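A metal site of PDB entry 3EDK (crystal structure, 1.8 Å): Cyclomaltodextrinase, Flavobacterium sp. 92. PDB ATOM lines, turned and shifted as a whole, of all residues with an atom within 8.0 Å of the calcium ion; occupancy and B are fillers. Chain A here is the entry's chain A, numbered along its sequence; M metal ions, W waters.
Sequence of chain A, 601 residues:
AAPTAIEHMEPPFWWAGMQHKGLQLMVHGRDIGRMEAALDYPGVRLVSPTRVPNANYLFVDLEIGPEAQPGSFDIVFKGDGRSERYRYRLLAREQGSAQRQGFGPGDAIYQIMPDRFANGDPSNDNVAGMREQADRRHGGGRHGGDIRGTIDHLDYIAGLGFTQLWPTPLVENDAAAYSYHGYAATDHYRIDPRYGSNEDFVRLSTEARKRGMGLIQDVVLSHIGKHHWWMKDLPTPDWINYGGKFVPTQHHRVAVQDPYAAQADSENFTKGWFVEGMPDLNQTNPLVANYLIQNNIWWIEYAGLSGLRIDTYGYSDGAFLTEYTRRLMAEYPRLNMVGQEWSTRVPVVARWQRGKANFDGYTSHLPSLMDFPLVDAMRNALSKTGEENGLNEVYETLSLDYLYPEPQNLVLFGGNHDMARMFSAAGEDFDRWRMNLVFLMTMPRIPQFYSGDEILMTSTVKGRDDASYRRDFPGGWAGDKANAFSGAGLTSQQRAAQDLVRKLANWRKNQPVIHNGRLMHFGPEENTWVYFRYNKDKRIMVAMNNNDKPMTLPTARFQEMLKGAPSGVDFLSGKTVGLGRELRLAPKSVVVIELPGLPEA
The backbone NH (N) of Gly 120 sits at hydrogen-bond distance from the side-chain carboxylate (OD2) of Asp 146 (2.9 Å).
The backbone NH (N) of Asp 146 is in hydrogen-bond range of the backbone carbonyl oxygen (O) of Ala 118, at 2.9 Å.
OD2 of Asp 146 sits at hydrogen-bond distance from N of Gly 149, at 2.8 Å.
N of Arg 148 lies close to OD2 of Asp 146, at 3.4 Å.
O of Pro 114 sits at hydrogen-bond distance from N of Asp 146 (3.4 Å).
The side-chain amide nitrogen (ND2) of Asn 124 lies close to the backbone carbonyl oxygen (O) of Arg 194 (3.4 Å).
The side-chain carboxylate of Asp 115 is in hydrogen-bond range of the backbone NH of Gly 144 (2.9 Å).
The side-chain amide nitrogen (ND2) of Asn 119 lies close to the indole nitrogen (NE1) of Trp 477 (3.4 Å).
Six residues have an atom within 4 Å of the calcium ion: Asn 119, Asp 121, Asn 124, Asp 125, Gly 144 and Asp 146.
The calcium ion is bound by OD1 of Asp 125 (2.3 Å), OD1 of Asp 146 (2.3 Å), OD1 of Asn 124 (2.4 Å), O of Gly 144 (2.4 Å), OD1 of Asn 119 (2.5 Å), O of Asp 121 (2.5 Å) and water W1 (2.6 Å).
The calcium ion has seven donor atoms within binding distance.
Water W1 lies within hydrogen-bond range of the backbone carbonyl oxygen of Arg 194 (2.6 Å) and the backbone carbonyl oxygen of Gly 145 (3.5 Å).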
ATOM      1  N   PRO A 114       7.420 -20.227  10.839  1.00  0.00           N
ATOM      2  CA  PRO A 114       8.630 -20.763  10.186  1.00  0.00           C
ATOM      3  C   PRO A 114       9.932 -20.125  10.705  1.00  0.00           C
ATOM      4  O   PRO A 114      10.917 -20.822  10.855  1.00  0.00           O
ATOM      5  CB  PRO A 114       8.413 -20.467   8.709  1.00  0.00           C
ATOM      6  CG  PRO A 114       7.250 -19.492   8.680  1.00  0.00           C
ATOM      7  CD  PRO A 114       6.422 -19.825   9.836  1.00  0.00           C
ATOM      8  N   ASP A 115       9.914 -18.827  11.020  1.00  0.00           N
ATOM      9  CA  ASP A 115      11.137 -18.204  11.601  1.00  0.00           C
ATOM     10  C   ASP A 115      11.513 -18.712  13.009  1.00  0.00           C
ATOM     11  O   ASP A 115      12.688 -18.583  13.438  1.00  0.00           O
ATOM     12  CB  ASP A 115      10.985 -16.678  11.668  1.00  0.00           C
ATOM     13  CG  ASP A 115      12.249 -15.995  12.144  1.00  0.00           C
ATOM     14  OD1 ASP A 115      12.229 -15.330  13.213  1.00  0.00           O
ATOM     15  OD2 ASP A 115      13.266 -16.169  11.441  1.00  0.00           O
ATOM     16  N   ALA A 118      12.625 -24.056  13.313  1.00  0.00           N
ATOM     17  CA  ALA A 118      13.905 -24.725  13.131  1.00  0.00           C
ATOM     18  C   ALA A 118      14.774 -24.052  12.066  1.00  0.00           C
ATOM     19  O   ALA A 118      14.362 -23.820  10.943  1.00  0.00           O
ATOM     20  CB  ALA A 118      13.721 -26.227  12.870  1.00  0.00           C
ATOM     21  N   ASN A 119      15.993 -23.725  12.476  1.00  0.00           N
ATOM     22  CA  ASN A 119      16.974 -23.087  11.610  1.00  0.00           C
ATOM     23  C   ASN A 119      17.873 -24.170  10.994  1.00  0.00           C
ATOM     24  O   ASN A 119      18.885 -24.551  11.563  1.00  0.00           O
ATOM     25  CB  ASN A 119      17.773 -22.061  12.423  1.00  0.00           C
ATOM     26  CG  ASN A 119      18.669 -21.189  11.542  1.00  0.00           C
ATOM     27  OD1 ASN A 119      18.823 -21.438  10.350  1.00  0.00           O
ATOM     28  ND2 ASN A 119      19.301 -20.166  12.155  1.00  0.00           N
ATOM     29  N   GLY A 120      17.461 -24.659   9.826  1.00  0.00           N
ATOM     30  CA  GLY A 120      18.124 -25.769   9.174  1.00  0.00           C
ATOM     31  C   GLY A 120      19.363 -25.269   8.450  1.00  0.00           C
ATOM     32  O   GLY A 120      20.277 -26.035   8.151  1.00  0.00           O
ATOM     33  N   ASP A 121      19.365 -23.968   8.159  1.00  0.00           N
ATOM     34  CA  ASP A 121      20.463 -23.372   7.396  1.00  0.00           C
ATOM     35  C   ASP A 121      20.766 -21.976   7.912  1.00  0.00           C
ATOM     36  O   ASP A 121      20.104 -21.029   7.498  1.00  0.00           O
ATOM     37  CB  ASP A 121      20.057 -23.292   5.927  1.00  0.00           C
ATOM     38  CG  ASP A 121      21.173 -22.817   5.040  1.00  0.00           C
ATOM     39  OD1 ASP A 121      22.265 -22.416   5.545  1.00  0.00           O
ATOM     40  OD2 ASP A 121      20.952 -22.842   3.826  1.00  0.00           O
ATOM     41  N   PRO A 122      21.778 -21.844   8.803  1.00  0.00           N
ATOM     42  CA  PRO A 122      22.128 -20.491   9.269  1.00  0.00           C
ATOM     43  C   PRO A 122      22.541 -19.516   8.178  1.00  0.00           C
ATOM     44  O   PRO A 122      22.451 -18.318   8.387  1.00  0.00           O
ATOM     45  CB  PRO A 122      23.287 -20.750  10.249  1.00  0.00           C
ATOM     46  CG  PRO A 122      23.002 -22.148  10.753  1.00  0.00           C
ATOM     47  CD  PRO A 122      22.582 -22.868   9.497  1.00  0.00           C
ATOM     48  N   SER A 123      22.964 -20.026   7.026  1.00  0.00           N
ATOM     49  CA  SER A 123      23.515 -19.156   5.973  1.00  0.00           C
ATOM     50  C   SER A 123      22.441 -18.296   5.300  1.00  0.00           C
ATOM     51  O   SER A 123      22.761 -17.306   4.673  1.00  0.00           O
ATOM     52  CB  SER A 123      24.293 -19.952   4.927  1.00  0.00           C
ATOM     53  OG  SER A 123      23.418 -20.594   4.015  1.00  0.00           O
ATOM     54  N   ASN A 124      21.175 -18.673   5.422  1.00  0.00           N
ATOM     55  CA  ASN A 124      20.129 -17.836   4.840  1.00  0.00           C
ATOM     56  C   ASN A 124      19.465 -16.903   5.858  1.00  0.00           C
ATOM     57  O   ASN A 124      18.498 -16.205   5.535  1.00  0.00           O
ATOM     58  CB  ASN A 124      19.097 -18.674   4.061  1.00  0.00           C
ATOM     59  CG  ASN A 124      18.305 -19.616   4.970  1.00  0.00           C
ATOM     60  OD1 ASN A 124      18.266 -19.474   6.189  1.00  0.00           O
ATOM     61  ND2 ASN A 124      17.661 -20.604   4.357  1.00  0.00           N
ATOM     62  N   ASP A 125      19.984 -16.895   7.089  1.00  0.00           N
ATOM     63  CA  ASP A 125      19.418 -16.027   8.158  1.00  0.00           C
ATOM     64  C   ASP A 125      19.381 -14.570   7.698  1.00  0.00           C
ATOM     65  O   ASP A 125      18.459 -13.827   8.049  1.00  0.00           O
ATOM     66  CB  ASP A 125      20.198 -16.130   9.473  1.00  0.00           C
ATOM     67  CG  ASP A 125      20.066 -17.497  10.130  1.00  0.00           C
ATOM     68  OD1 ASP A 125      19.438 -18.407   9.532  1.00  0.00           O
ATOM     69  OD2 ASP A 125      20.604 -17.680  11.255  1.00  0.00           O
ATOM     70  N   ASN A 126      20.428 -14.171   6.960  1.00  0.00           N
ATOM     71  CA  ASN A 126      20.507 -12.907   6.263  1.00  0.00           C
ATOM     72  C   ASN A 126      20.679 -13.190   4.793  1.00  0.00           C
ATOM     73  O   ASN A 126      21.313 -14.183   4.402  1.00  0.00           O
ATOM     74  CB  ASN A 126      21.692 -12.068   6.765  1.00  0.00           C
ATOM     75  CG  ASN A 126      21.532 -11.674   8.213  1.00  0.00           C
ATOM     76  OD1 ASN A 126      20.491 -11.157   8.606  1.00  0.00           O
ATOM     77  ND2 ASN A 126      22.552 -11.942   9.024  1.00  0.00           N
ATOM     78  N   ALA A 134      19.167 -10.431  10.886  1.00  0.00           N
ATOM     79  CA  ALA A 134      18.682 -11.355  11.909  1.00  0.00           C
ATOM     80  C   ALA A 134      19.239 -11.011  13.288  1.00  0.00           C
ATOM     81  O   ALA A 134      20.380 -10.538  13.413  1.00  0.00           O
ATOM     82  CB  ALA A 134      19.042 -12.794  11.547  1.00  0.00           C
ATOM     83  N   ARG A 142      14.193 -11.368  13.432  1.00  0.00           N
ATOM     84  CA  ARG A 142      14.299 -12.665  12.753  1.00  0.00           C
ATOM     85  C   ARG A 142      15.289 -13.557  13.513  1.00  0.00           C
ATOM     86  O   ARG A 142      16.437 -13.153  13.797  1.00  0.00           O
ATOM     87  CB  ARG A 142      14.759 -12.523  11.316  1.00  0.00           C
ATOM     88  CG  ARG A 142      13.851 -11.686  10.440  1.00  0.00           C
ATOM     89  CD  ARG A 142      14.238 -11.863   8.980  1.00  0.00           C
ATOM     90  NE  ARG A 142      13.885 -13.203   8.510  1.00  0.00           N
ATOM     91  CZ  ARG A 142      12.727 -13.509   7.928  1.00  0.00           C
ATOM     92  NH1 ARG A 142      12.484 -14.747   7.516  1.00  0.00           N
ATOM     93  NH2 ARG A 142      11.813 -12.550   7.771  1.00  0.00           N
ATOM     94  N   HIS A 143      14.860 -14.781  13.820  1.00  0.00           N
ATOM     95  CA  HIS A 143      15.700 -15.730  14.551  1.00  0.00           C
ATOM     96  C   HIS A 143      16.415 -16.733  13.652  1.00  0.00           C
ATOM     97  O   HIS A 143      17.458 -17.320  14.041  1.00  0.00           O
ATOM     98  CB  HIS A 143      14.862 -16.422  15.652  1.00  0.00           C
ATOM     99  CG  HIS A 143      14.382 -15.467  16.707  1.00  0.00           C
ATOM    100  ND1 HIS A 143      13.720 -15.886  17.842  1.00  0.00           N
ATOM    101  CD2 HIS A 143      14.487 -14.114  16.813  1.00  0.00           C
ATOM    102  CE1 HIS A 143      13.425 -14.846  18.592  1.00  0.00           C
ATOM    103  NE2 HIS A 143      13.886 -13.755  17.998  1.00  0.00           N
ATOM    104  N   GLY A 144      15.846 -16.932  12.464  1.00  0.00           N
ATOM    105  CA  GLY A 144      16.503 -17.688  11.402  1.00  0.00           C
ATOM    106  C   GLY A 144      15.858 -19.013  11.026  1.00  0.00           C
ATOM    107  O   GLY A 144      16.430 -19.788  10.274  1.00  0.00           O
ATOM    108  N   GLY A 145      14.666 -19.266  11.553  1.00  0.00           N
ATOM    109  CA  GLY A 145      13.949 -20.487  11.152  1.00  0.00           C
ATOM    110  C   GLY A 145      13.710 -20.489   9.649  1.00  0.00           C
ATOM    111  O   GLY A 145      13.477 -19.449   9.035  1.00  0.00           O
ATOM    112  N   ASP A 146      13.723 -21.671   9.042  1.00  0.00           N
ATOM    113  CA  ASP A 146      13.583 -21.760   7.591  1.00  0.00           C
ATOM    114  C   ASP A 146      12.945 -23.064   7.133  1.00  0.00           C
ATOM    115  O   ASP A 146      12.641 -23.936   7.938  1.00  0.00           O
ATOM    116  CB  ASP A 146      14.957 -21.547   6.940  1.00  0.00           C
ATOM    117  CG  ASP A 146      16.020 -22.475   7.558  1.00  0.00           C
ATOM    118  OD1 ASP A 146      17.163 -22.013   7.835  1.00  0.00           O
ATOM    119  OD2 ASP A 146      15.701 -23.656   7.791  1.00  0.00           O
ATOM    120  N   ILE A 147      12.773 -23.202   5.814  1.00  0.00           N
ATOM    121  CA  ILE A 147      12.128 -24.390   5.224  1.00  0.00           C
ATOM    122  C   ILE A 147      12.963 -25.661   5.455  1.00  0.00           C
ATOM    123  O   ILE A 147      12.433 -26.704   5.762  1.00  0.00           O
ATOM    124  CB  ILE A 147      11.817 -24.189   3.722  1.00  0.00           C
ATOM    125  CG1 ILE A 147      10.688 -23.155   3.564  1.00  0.00           C
ATOM    126  CG2 ILE A 147      11.452 -25.531   3.045  1.00  0.00           C
ATOM    127  CD1 ILE A 147      10.543 -22.640   2.157  1.00  0.00           C
ATOM    128  N   ARG A 148      14.290 -25.550   5.293  1.00  0.00           N
ATOM    129  CA  ARG A 148      15.163 -26.688   5.591  1.00  0.00           C
ATOM    130  C   ARG A 148      14.964 -27.245   7.006  1.00  0.00           C
ATOM    131  O   ARG A 148      14.870 -28.468   7.191  1.00  0.00           O
ATOM    132  CB  ARG A 148      16.638 -26.286   5.356  1.00  0.00           C
ATOM    133  CG  ARG A 148      17.636 -27.424   5.673  1.00  0.00           C
ATOM    134  CD  ARG A 148      18.979 -27.142   5.043  1.00  0.00           C
ATOM    135  NE  ARG A 148      19.997 -28.079   5.508  1.00  0.00           N
ATOM    136  CZ  ARG A 148      21.292 -27.985   5.251  1.00  0.00           C
ATOM    137  NH1 ARG A 148      22.132 -28.899   5.742  1.00  0.00           N
ATOM    138  NH2 ARG A 148      21.770 -26.995   4.500  1.00  0.00           N
ATOM    139  N   GLY A 149      14.899 -26.363   8.001  1.00  0.00           N
ATOM    140  CA  GLY A 149      14.653 -26.757   9.387  1.00  0.00           C
ATOM    141  C   GLY A 149      13.289 -27.412   9.560  1.00  0.00           C
ATOM    142  O   GLY A 149      13.151 -28.427  10.241  1.00  0.00           O
ATOM    143  N   PRO A 193      13.438 -15.157   0.753  1.00  0.00           N
ATOM    144  CA  PRO A 193      14.689 -15.899   0.557  1.00  0.00           C
ATOM    145  C   PRO A 193      15.338 -16.364   1.877  1.00  0.00           C
ATOM    146  O   PRO A 193      16.141 -17.284   1.894  1.00  0.00           O
ATOM    147  CB  PRO A 193      15.614 -14.894  -0.177  1.00  0.00           C
ATOM    148  CG  PRO A 193      14.761 -13.849  -0.701  1.00  0.00           C
ATOM    149  CD  PRO A 193      13.470 -13.822   0.122  1.00  0.00           C
ATOM    150  N   ARG A 194      14.964 -15.744   2.975  1.00  0.00           N
ATOM    151  CA  ARG A 194      15.488 -16.187   4.230  1.00  0.00           C
ATOM    152  C   ARG A 194      14.884 -17.518   4.677  1.00  0.00           C
ATOM    153  O   ARG A 194      15.482 -18.213   5.486  1.00  0.00           O
ATOM    154  CB  ARG A 194      15.365 -15.096   5.273  1.00  0.00           C
ATOM    155  CG  ARG A 194      16.269 -13.918   4.867  1.00  0.00           C
ATOM    156  CD  ARG A 194      15.934 -12.717   5.625  1.00  0.00           C
ATOM    157  NE  ARG A 194      14.616 -12.186   5.262  1.00  0.00           N
ATOM    158  CZ  ARG A 194      14.241 -10.947   5.543  1.00  0.00           C
ATOM    159  NH1 ARG A 194      15.099 -10.109   6.160  1.00  0.00           N
ATOM    160  NH2 ARG A 194      13.022 -10.528   5.205  1.00  0.00           N
ATOM    161  N   TYR A 195      13.724 -17.854   4.123  1.00  0.00           N
ATOM    162  CA  TYR A 195      13.129 -19.168   4.384  1.00  0.00           C
ATOM    163  C   TYR A 195      13.620 -20.207   3.389  1.00  0.00           C
ATOM    164  O   TYR A 195      13.668 -21.392   3.714  1.00  0.00           O
ATOM    165  CB  TYR A 195      11.598 -19.108   4.343  1.00  0.00           C
ATOM    166  CG  TYR A 195      11.009 -18.291   5.463  1.00  0.00           C
ATOM    167  CD1 TYR A 195      11.389 -18.495   6.788  1.00  0.00           C
ATOM    168  CD2 TYR A 195      10.129 -17.251   5.176  1.00  0.00           C
ATOM    169  CE1 TYR A 195      10.855 -17.746   7.822  1.00  0.00           C
ATOM    170  CE2 TYR A 195       9.578 -16.485   6.206  1.00  0.00           C
ATOM    171  CZ  TYR A 195       9.957 -16.743   7.532  1.00  0.00           C
ATOM    172  OH  TYR A 195       9.452 -15.970   8.568  1.00  0.00           O
ATOM    173  N   GLY A 196      13.943 -19.743   2.175  1.00  0.00           N
ATOM    174  CA  GLY A 196      14.332 -20.588   1.058  1.00  0.00           C
ATOM    175  C   GLY A 196      13.723 -20.135  -0.261  1.00  0.00           C
ATOM    176  O   GLY A 196      13.342 -18.971  -0.433  1.00  0.00           O
ATOM    177  N   TRP A 477      17.676 -24.864  16.909  1.00  0.00           N
ATOM    178  CA  TRP A 477      18.927 -24.122  16.652  1.00  0.00           C
ATOM    179  C   TRP A 477      20.111 -24.924  17.160  1.00  0.00           C
ATOM    180  O   TRP A 477      20.072 -25.482  18.259  1.00  0.00           O
ATOM    181  CB  TRP A 477      18.925 -22.749  17.338  1.00  0.00           C
ATOM    182  CG  TRP A 477      18.248 -21.701  16.545  1.00  0.00           C
ATOM    183  CD1 TRP A 477      18.848 -20.695  15.839  1.00  0.00           C
ATOM    184  CD2 TRP A 477      16.836 -21.577  16.305  1.00  0.00           C
ATOM    185  NE1 TRP A 477      17.889 -19.941  15.194  1.00  0.00           N
ATOM    186  CE2 TRP A 477      16.649 -20.472  15.455  1.00  0.00           C
ATOM    187  CE3 TRP A 477      15.698 -22.297  16.747  1.00  0.00           C
ATOM    188  CZ2 TRP A 477      15.372 -20.053  15.024  1.00  0.00           C
ATOM    189  CZ3 TRP A 477      14.420 -21.883  16.300  1.00  0.00           C
ATOM    190  CH2 TRP A 477      14.274 -20.763  15.465  1.00  0.00           C
HETATM  191 CA    CA M   1      18.077 -19.966   8.508  1.00  0.00          CA
HETATM  192  O   HOH W   1      16.461 -18.043   7.923  1.00  0.00           O
